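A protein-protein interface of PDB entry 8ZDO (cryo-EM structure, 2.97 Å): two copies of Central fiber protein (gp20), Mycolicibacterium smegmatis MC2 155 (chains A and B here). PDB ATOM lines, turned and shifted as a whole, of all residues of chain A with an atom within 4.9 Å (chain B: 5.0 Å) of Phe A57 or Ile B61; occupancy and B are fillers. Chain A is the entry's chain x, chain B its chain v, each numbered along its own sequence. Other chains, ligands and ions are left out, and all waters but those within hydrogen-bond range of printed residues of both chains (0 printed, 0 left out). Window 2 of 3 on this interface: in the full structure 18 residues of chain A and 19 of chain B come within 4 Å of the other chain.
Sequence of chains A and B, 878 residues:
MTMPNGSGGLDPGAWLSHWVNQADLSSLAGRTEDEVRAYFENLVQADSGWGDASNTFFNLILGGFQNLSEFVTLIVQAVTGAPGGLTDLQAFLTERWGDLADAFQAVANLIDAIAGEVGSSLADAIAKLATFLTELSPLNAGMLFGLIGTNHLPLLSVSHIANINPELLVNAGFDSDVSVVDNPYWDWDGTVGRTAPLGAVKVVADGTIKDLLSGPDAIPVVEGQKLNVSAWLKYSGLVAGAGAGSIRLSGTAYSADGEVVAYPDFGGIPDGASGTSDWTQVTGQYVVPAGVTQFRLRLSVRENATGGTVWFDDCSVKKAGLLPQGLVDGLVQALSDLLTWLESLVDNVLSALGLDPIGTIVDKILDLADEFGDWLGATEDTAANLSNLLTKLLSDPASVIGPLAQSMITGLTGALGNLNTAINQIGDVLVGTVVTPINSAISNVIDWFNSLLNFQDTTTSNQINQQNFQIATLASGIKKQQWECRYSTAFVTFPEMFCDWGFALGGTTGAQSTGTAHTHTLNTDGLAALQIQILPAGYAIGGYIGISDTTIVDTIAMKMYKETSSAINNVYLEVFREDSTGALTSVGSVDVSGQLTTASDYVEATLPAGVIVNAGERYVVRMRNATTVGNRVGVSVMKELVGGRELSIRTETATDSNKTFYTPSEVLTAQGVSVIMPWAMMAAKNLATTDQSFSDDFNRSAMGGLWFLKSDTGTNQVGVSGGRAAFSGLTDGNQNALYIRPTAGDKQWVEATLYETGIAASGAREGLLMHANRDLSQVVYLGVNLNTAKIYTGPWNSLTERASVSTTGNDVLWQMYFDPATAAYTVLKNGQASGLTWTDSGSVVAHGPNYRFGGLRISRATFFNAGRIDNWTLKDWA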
ATOM      1  N   ALA A  53      20.397  23.382 -28.168  1.00  0.00           N
ATOM      2  CA  ALA A  53      19.296  22.451 -27.960  1.00  0.00           C
ATOM      3  C   ALA A  53      17.985  23.193 -27.743  1.00  0.00           C
ATOM      4  O   ALA A  53      16.936  22.770 -28.240  1.00  0.00           O
ATOM      5  CB  ALA A  53      19.601  21.536 -26.777  1.00  0.00           C
ATOM      6  N   SER A  54      18.023  24.296 -26.993  1.00  0.00           N
ATOM      7  CA  SER A  54      16.821  25.095 -26.787  1.00  0.00           C
ATOM      8  C   SER A  54      16.308  25.664 -28.099  1.00  0.00           C
ATOM      9  O   SER A  54      15.100  25.642 -28.365  1.00  0.00           O
ATOM     10  CB  SER A  54      17.105  26.217 -25.790  1.00  0.00           C
ATOM     11  OG  SER A  54      15.940  26.978 -25.539  1.00  0.00           O
ATOM     12  N   ASN A  55      17.213  26.179 -28.934  1.00  0.00           N
ATOM     13  CA  ASN A  55      16.809  26.692 -30.238  1.00  0.00           C
ATOM     14  C   ASN A  55      16.157  25.597 -31.070  1.00  0.00           C
ATOM     15  O   ASN A  55      15.080  25.793 -31.644  1.00  0.00           O
ATOM     16  CB  ASN A  55      18.015  27.274 -30.973  1.00  0.00           C
ATOM     17  CG  ASN A  55      18.509  28.562 -30.356  1.00  0.00           C
ATOM     18  OD1 ASN A  55      17.832  29.167 -29.525  1.00  0.00           O
ATOM     19  ND2 ASN A  55      19.699  28.991 -30.759  1.00  0.00           N
ATOM     20  N   THR A  56      16.788  24.422 -31.120  1.00  0.00           N
ATOM     21  CA  THR A  56      16.253  23.320 -31.912  1.00  0.00           C
ATOM     22  C   THR A  56      14.885  22.885 -31.405  1.00  0.00           C
ATOM     23  O   THR A  56      13.968  22.646 -32.198  1.00  0.00           O
ATOM     24  CB  THR A  56      17.226  22.142 -31.892  1.00  0.00           C
ATOM     25  OG1 THR A  56      18.460  22.528 -32.507  1.00  0.00           O
ATOM     26  CG2 THR A  56      16.644  20.955 -32.638  1.00  0.00           C
ATOM     27  N   PHE A  57      14.725  22.783 -30.086  1.00  0.00           N
ATOM     28  CA  PHE A  57      13.469  22.299 -29.526  1.00  0.00           C
ATOM     29  C   PHE A  57      12.346  23.305 -29.726  1.00  0.00           C
ATOM     30  O   PHE A  57      11.255  22.947 -30.182  1.00  0.00           O
ATOM     31  CB  PHE A  57      13.649  21.984 -28.044  1.00  0.00           C
ATOM     32  CG  PHE A  57      12.435  21.385 -27.399  1.00  0.00           C
ATOM     33  CD1 PHE A  57      12.025  20.106 -27.717  1.00  0.00           C
ATOM     34  CD2 PHE A  57      11.705  22.102 -26.468  1.00  0.00           C
ATOM     35  CE1 PHE A  57      10.911  19.554 -27.125  1.00  0.00           C
ATOM     36  CE2 PHE A  57      10.591  21.556 -25.872  1.00  0.00           C
ATOM     37  CZ  PHE A  57      10.194  20.280 -26.202  1.00  0.00           C
ATOM     38  N   PHE A  58      12.589  24.572 -29.398  1.00  0.00           N
ATOM     39  CA  PHE A  58      11.524  25.561 -29.395  1.00  0.00           C
ATOM     40  C   PHE A  58      11.307  26.226 -30.746  1.00  0.00           C
ATOM     41  O   PHE A  58      10.333  26.970 -30.895  1.00  0.00           O
ATOM     42  CB  PHE A  58      11.807  26.636 -28.342  1.00  0.00           C
ATOM     43  CG  PHE A  58      11.711  26.133 -26.936  1.00  0.00           C
ATOM     44  CD1 PHE A  58      10.486  25.799 -26.391  1.00  0.00           C
ATOM     45  CD2 PHE A  58      12.845  25.988 -26.160  1.00  0.00           C
ATOM     46  CE1 PHE A  58      10.395  25.332 -25.099  1.00  0.00           C
ATOM     47  CE2 PHE A  58      12.759  25.523 -24.869  1.00  0.00           C
ATOM     48  CZ  PHE A  58      11.533  25.195 -24.337  1.00  0.00           C
ATOM     49  N   ASN A  59      12.168  25.986 -31.725  1.00  0.00           N
ATOM     50  CA  ASN A  59      11.995  26.586 -33.040  1.00  0.00           C
ATOM     51  C   ASN A  59      11.815  25.564 -34.148  1.00  0.00           C
ATOM     52  O   ASN A  59      10.983  25.766 -35.034  1.00  0.00           O
ATOM     53  CB  ASN A  59      13.188  27.491 -33.368  1.00  0.00           C
ATOM     54  CG  ASN A  59      13.323  28.645 -32.399  1.00  0.00           C
ATOM     55  OD1 ASN A  59      12.337  29.293 -32.050  1.00  0.00           O
ATOM     56  ND2 ASN A  59      14.546  28.907 -31.956  1.00  0.00           N
ATOM     57  N   LEU A  60      12.567  24.466 -34.121  1.00  0.00           N
ATOM     58  CA  LEU A  60      12.429  23.435 -35.142  1.00  0.00           C
ATOM     59  C   LEU A  60      11.352  22.421 -34.769  1.00  0.00           C
ATOM     60  O   LEU A  60      10.375  22.252 -35.502  1.00  0.00           O
ATOM     61  CB  LEU A  60      13.775  22.738 -35.373  1.00  0.00           C
ATOM     62  CG  LEU A  60      13.737  21.375 -36.066  1.00  0.00           C
ATOM     63  CD1 LEU A  60      13.281  21.515 -37.507  1.00  0.00           C
ATOM     64  CD2 LEU A  60      15.098  20.706 -35.997  1.00  0.00           C
ATOM     65  N   ILE A  61      11.511  21.753 -33.625  1.00  0.00           N
ATOM     66  CA  ILE A  61      10.592  20.680 -33.252  1.00  0.00           C
ATOM     67  C   ILE A  61       9.211  21.238 -32.942  1.00  0.00           C
ATOM     68  O   ILE A  61       8.192  20.715 -33.409  1.00  0.00           O
ATOM     69  CB  ILE A  61      11.155  19.881 -32.066  1.00  0.00           C
ATOM     70  CG1 ILE A  61      12.425  19.145 -32.482  1.00  0.00           C
ATOM     71  CG2 ILE A  61      10.122  18.899 -31.548  1.00  0.00           C
ATOM     72  CD1 ILE A  61      13.155  18.518 -31.337  1.00  0.00           C
ATOM     73  N   LEU A  62       9.151  22.304 -32.151  1.00  0.00           N
ATOM     74  CA  LEU A  62       7.883  22.896 -31.756  1.00  0.00           C
ATOM     75  C   LEU A  62       7.402  23.966 -32.722  1.00  0.00           C
ATOM     76  O   LEU A  62       6.344  24.558 -32.488  1.00  0.00           O
ATOM     77  CB  LEU A  62       7.993  23.492 -30.350  1.00  0.00           C
ATOM     78  CG  LEU A  62       8.041  22.507 -29.185  1.00  0.00           C
ATOM     79  CD1 LEU A  62       8.176  23.256 -27.876  1.00  0.00           C
ATOM     80  CD2 LEU A  62       6.806  21.631 -29.173  1.00  0.00           C
ATOM     81  N   GLN A  66       4.783  28.005 -28.779  1.00  0.00           N
ATOM     82  CA  GLN A  66       5.362  27.728 -27.471  1.00  0.00           C
ATOM     83  C   GLN A  66       4.991  26.332 -26.984  1.00  0.00           C
ATOM     84  O   GLN A  66       5.840  25.611 -26.447  1.00  0.00           O
ATOM     85  CB  GLN A  66       4.910  28.785 -26.465  1.00  0.00           C
ATOM     86  CG  GLN A  66       5.475  30.175 -26.723  1.00  0.00           C
ATOM     87  CD  GLN A  66       4.692  30.943 -27.772  1.00  0.00           C
ATOM     88  OE1 GLN A  66       4.565  30.506 -28.916  1.00  0.00           O
ATOM     89  NE2 GLN A  66       4.162  32.097 -27.384  1.00  0.00           N
ATOM     90  N   ASN A  67       3.737  25.932 -27.167  1.00  0.00           N
ATOM     91  CA  ASN A  67       3.269  24.659 -26.637  1.00  0.00           C
ATOM     92  C   ASN A  67       2.038  24.213 -27.411  1.00  0.00           C
ATOM     93  O   ASN A  67       1.468  24.960 -28.211  1.00  0.00           O
ATOM     94  CB  ASN A  67       2.966  24.759 -25.142  1.00  0.00           C
ATOM     95  CG  ASN A  67       2.055  25.921 -24.809  1.00  0.00           C
ATOM     96  OD1 ASN A  67       0.925  25.994 -25.287  1.00  0.00           O
ATOM     97  ND2 ASN A  67       2.543  26.837 -23.982  1.00  0.00           N
ATOM     98  N   LEU A  68       1.629  22.970 -27.145  1.00  0.00           N
ATOM     99  CA  LEU A  68       0.477  22.407 -27.834  1.00  0.00           C
ATOM    100  C   LEU A  68      -0.810  23.140 -27.489  1.00  0.00           C
ATOM    101  O   LEU A  68      -1.717  23.199 -28.318  1.00  0.00           O
ATOM    102  CB  LEU A  68       0.342  20.919 -27.512  1.00  0.00           C
ATOM    103  CG  LEU A  68       1.237  19.972 -28.308  1.00  0.00           C
ATOM    104  CD1 LEU A  68       0.728  18.547 -28.199  1.00  0.00           C
ATOM    105  CD2 LEU A  68       1.323  20.406 -29.760  1.00  0.00           C
ATOM    106  N   SER A  69      -0.913  23.709 -26.286  1.00  0.00           N
ATOM    107  CA  SER A  69      -2.115  24.462 -25.934  1.00  0.00           C
ATOM    108  C   SER A  69      -2.252  25.711 -26.800  1.00  0.00           C
ATOM    109  O   SER A  69      -3.319  25.971 -27.375  1.00  0.00           O
ATOM    110  CB  SER A  69      -2.080  24.834 -24.453  1.00  0.00           C
ATOM    111  OG  SER A  69      -1.897  23.687 -23.644  1.00  0.00           O
ATOM    112  N   THR B  56       6.244  19.775 -16.472  1.00  0.00           N
ATOM    113  CA  THR B  56       6.350  20.843 -17.461  1.00  0.00           C
ATOM    114  C   THR B  56       6.219  20.302 -18.879  1.00  0.00           C
ATOM    115  O   THR B  56       5.539  20.902 -19.719  1.00  0.00           O
ATOM    116  CB  THR B  56       7.679  21.579 -17.293  1.00  0.00           C
ATOM    117  OG1 THR B  56       7.765  22.113 -15.967  1.00  0.00           O
ATOM    118  CG2 THR B  56       7.790  22.711 -18.297  1.00  0.00           C
ATOM    119  N   PHE B  57       6.859  19.170 -19.164  1.00  0.00           N
ATOM    120  CA  PHE B  57       6.839  18.621 -20.513  1.00  0.00           C
ATOM    121  C   PHE B  57       5.453  18.117 -20.888  1.00  0.00           C
ATOM    122  O   PHE B  57       4.934  18.441 -21.962  1.00  0.00           O
ATOM    123  CB  PHE B  57       7.868  17.501 -20.635  1.00  0.00           C
ATOM    124  CG  PHE B  57       7.938  16.887 -22.001  1.00  0.00           C
ATOM    125  CD1 PHE B  57       8.427  17.605 -23.073  1.00  0.00           C
ATOM    126  CD2 PHE B  57       7.517  15.587 -22.209  1.00  0.00           C
ATOM    127  CE1 PHE B  57       8.493  17.039 -24.328  1.00  0.00           C
ATOM    128  CE2 PHE B  57       7.581  15.017 -23.461  1.00  0.00           C
ATOM    129  CZ  PHE B  57       8.070  15.745 -24.521  1.00  0.00           C
ATOM    130  N   ASN B  59       2.406  18.530 -19.311  1.00  0.00           N
ATOM    131  CA  ASN B  59       1.247  19.375 -19.052  1.00  0.00           C
ATOM    132  C   ASN B  59       1.333  20.719 -19.762  1.00  0.00           C
ATOM    133  O   ASN B  59       0.362  21.151 -20.388  1.00  0.00           O
ATOM    134  CB  ASN B  59       1.084  19.590 -17.543  1.00  0.00           C
ATOM    135  CG  ASN B  59       0.846  18.297 -16.795  1.00  0.00           C
ATOM    136  OD1 ASN B  59      -0.015  17.501 -17.169  1.00  0.00           O
ATOM    137  ND2 ASN B  59       1.610  18.078 -15.732  1.00  0.00           N
ATOM    138  N   LEU B  60       2.480  21.391 -19.683  1.00  0.00           N
ATOM    139  CA  LEU B  60       2.620  22.691 -20.328  1.00  0.00           C
ATOM    140  C   LEU B  60       2.944  22.545 -21.812  1.00  0.00           C
ATOM    141  O   LEU B  60       2.181  22.996 -22.671  1.00  0.00           O
ATOM    142  CB  LEU B  60       3.695  23.519 -19.618  1.00  0.00           C
ATOM    143  CG  LEU B  60       4.240  24.729 -20.375  1.00  0.00           C
ATOM    144  CD1 LEU B  60       3.192  25.825 -20.458  1.00  0.00           C
ATOM    145  CD2 LEU B  60       5.504  25.244 -19.713  1.00  0.00           C
ATOM    146  N   ILE B  61       4.072  21.905 -22.127  1.00  0.00           N
ATOM    147  CA  ILE B  61       4.532  21.847 -23.511  1.00  0.00           C
ATOM    148  C   ILE B  61       3.590  21.008 -24.364  1.00  0.00           C
ATOM    149  O   ILE B  61       3.245  21.388 -25.489  1.00  0.00           O
ATOM    150  CB  ILE B  61       5.975  21.314 -23.570  1.00  0.00           C
ATOM    151  CG1 ILE B  61       6.930  22.319 -22.934  1.00  0.00           C
ATOM    152  CG2 ILE B  61       6.383  21.034 -25.002  1.00  0.00           C
ATOM    153  CD1 ILE B  61       8.352  21.848 -22.886  1.00  0.00           C
ATOM    154  N   LEU B  62       3.153  19.862 -23.850  1.00  0.00           N
ATOM    155  CA  LEU B  62       2.313  18.946 -24.605  1.00  0.00           C
ATOM    156  C   LEU B  62       0.828  19.147 -24.343  1.00  0.00           C
ATOM    157  O   LEU B  62       0.016  18.354 -24.828  1.00  0.00           O
ATOM    158  CB  LEU B  62       2.700  17.499 -24.295  1.00  0.00           C
ATOM    159  CG  LEU B  62       3.959  16.974 -24.984  1.00  0.00           C
ATOM    160  CD1 LEU B  62       4.228  15.545 -24.569  1.00  0.00           C
ATOM    161  CD2 LEU B  62       3.825  17.077 -26.491  1.00  0.00           C
ATOM    162  N   GLY B  63       0.454  20.186 -23.599  1.00  0.00           N
ATOM    163  CA  GLY B  63      -0.951  20.384 -23.280  1.00  0.00           C
ATOM    164  C   GLY B  63      -1.473  19.260 -22.408  1.00  0.00           C
ATOM    165  O   GLY B  63      -0.803  18.794 -21.482  1.00  0.00           O
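The backbone carbonyl oxygen (O) of Ile B61 sits at hydrogen-bond distance from the backbone NH (N) of Leu A68, at 2.8 Å.
The backbone carbonyl oxygen of Thr B56 sits at hydrogen-bond distance from the backbone NH of Ile B61 (3.0 Å).
The backbone NH (N) of Leu A62 is in hydrogen-bond range of the backbone carbonyl oxygen (O) of Phe A57, at 3.0 Å.
N of Ser A69 sits at hydrogen-bond distance from OD1 of Asn A67 (3.1 Å).
The backbone carbonyl oxygen (O) of Phe B57 sits at hydrogen-bond distance from the backbone NH (N) of Leu B62 (3.0 Å).
Among the printed residues, pairs that only touch across the chains: Phe A57 with Ile B61, Asn A67 with Leu B60, Asn A67 with Ile B61, Leu A68 with Leu B62, Leu A68 with Gly B63 and Ser A69 with Gly B63.
Of chain B, only Ile B61 (3.7 Å) comes within 4 Å of Phe A57.
Ile B61 touches just these residues of chain A: Phe A57 (3.7 Å), Asn A67 (3.4 Å) and Leu A68 (2.8 Å).
Of the printed residues of chain A, Leu B62 touches Leu A68 (3.5 Å).
Of the printed residues of chain A, Gly B63 touches Leu A68 and Ser A69.
Printed residues of chain B within 4 Å of Ser A69: Gly B63 (3.5 Å).
Of the printed residues of chain B, Leu A68 touches Ile B61, Leu B62 and Gly B63.
Printed residues of chain B within 4 Å of Asn A67: Leu B60 and Ile B61.
Gln A66 touches none of the printed residues of chain B.
Leu A60 touches none of the printed residues of chain B.
The nearest residue of chain B that does not touch Phe A57 is Phe B57 (4.1 Å).
The nearest printed residue of chain B that does not touch Asn A67 is Leu B62 (5.1 Å).
Hydrophobic or aromatic side chains of chain B that line the printed part of chain A: Leu B60, Ile B61 and Leu B62.
Among the printed residues, 7 pairs touch across the chains.
Among the printed residues, no Asp or Glu carboxylate lies within 4 Å of a Lys or Arg side-chain nitrogen of the other chain.
Phe A57 touches Ile B61, but with the chains exchanged Ile A61 does not touch Phe B57 (7.6 Å).
6 positions are printed for both chains.
Of the 7 pairs that touch across the chains among the printed residues, none has its exchanged pair printed and touching as well.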
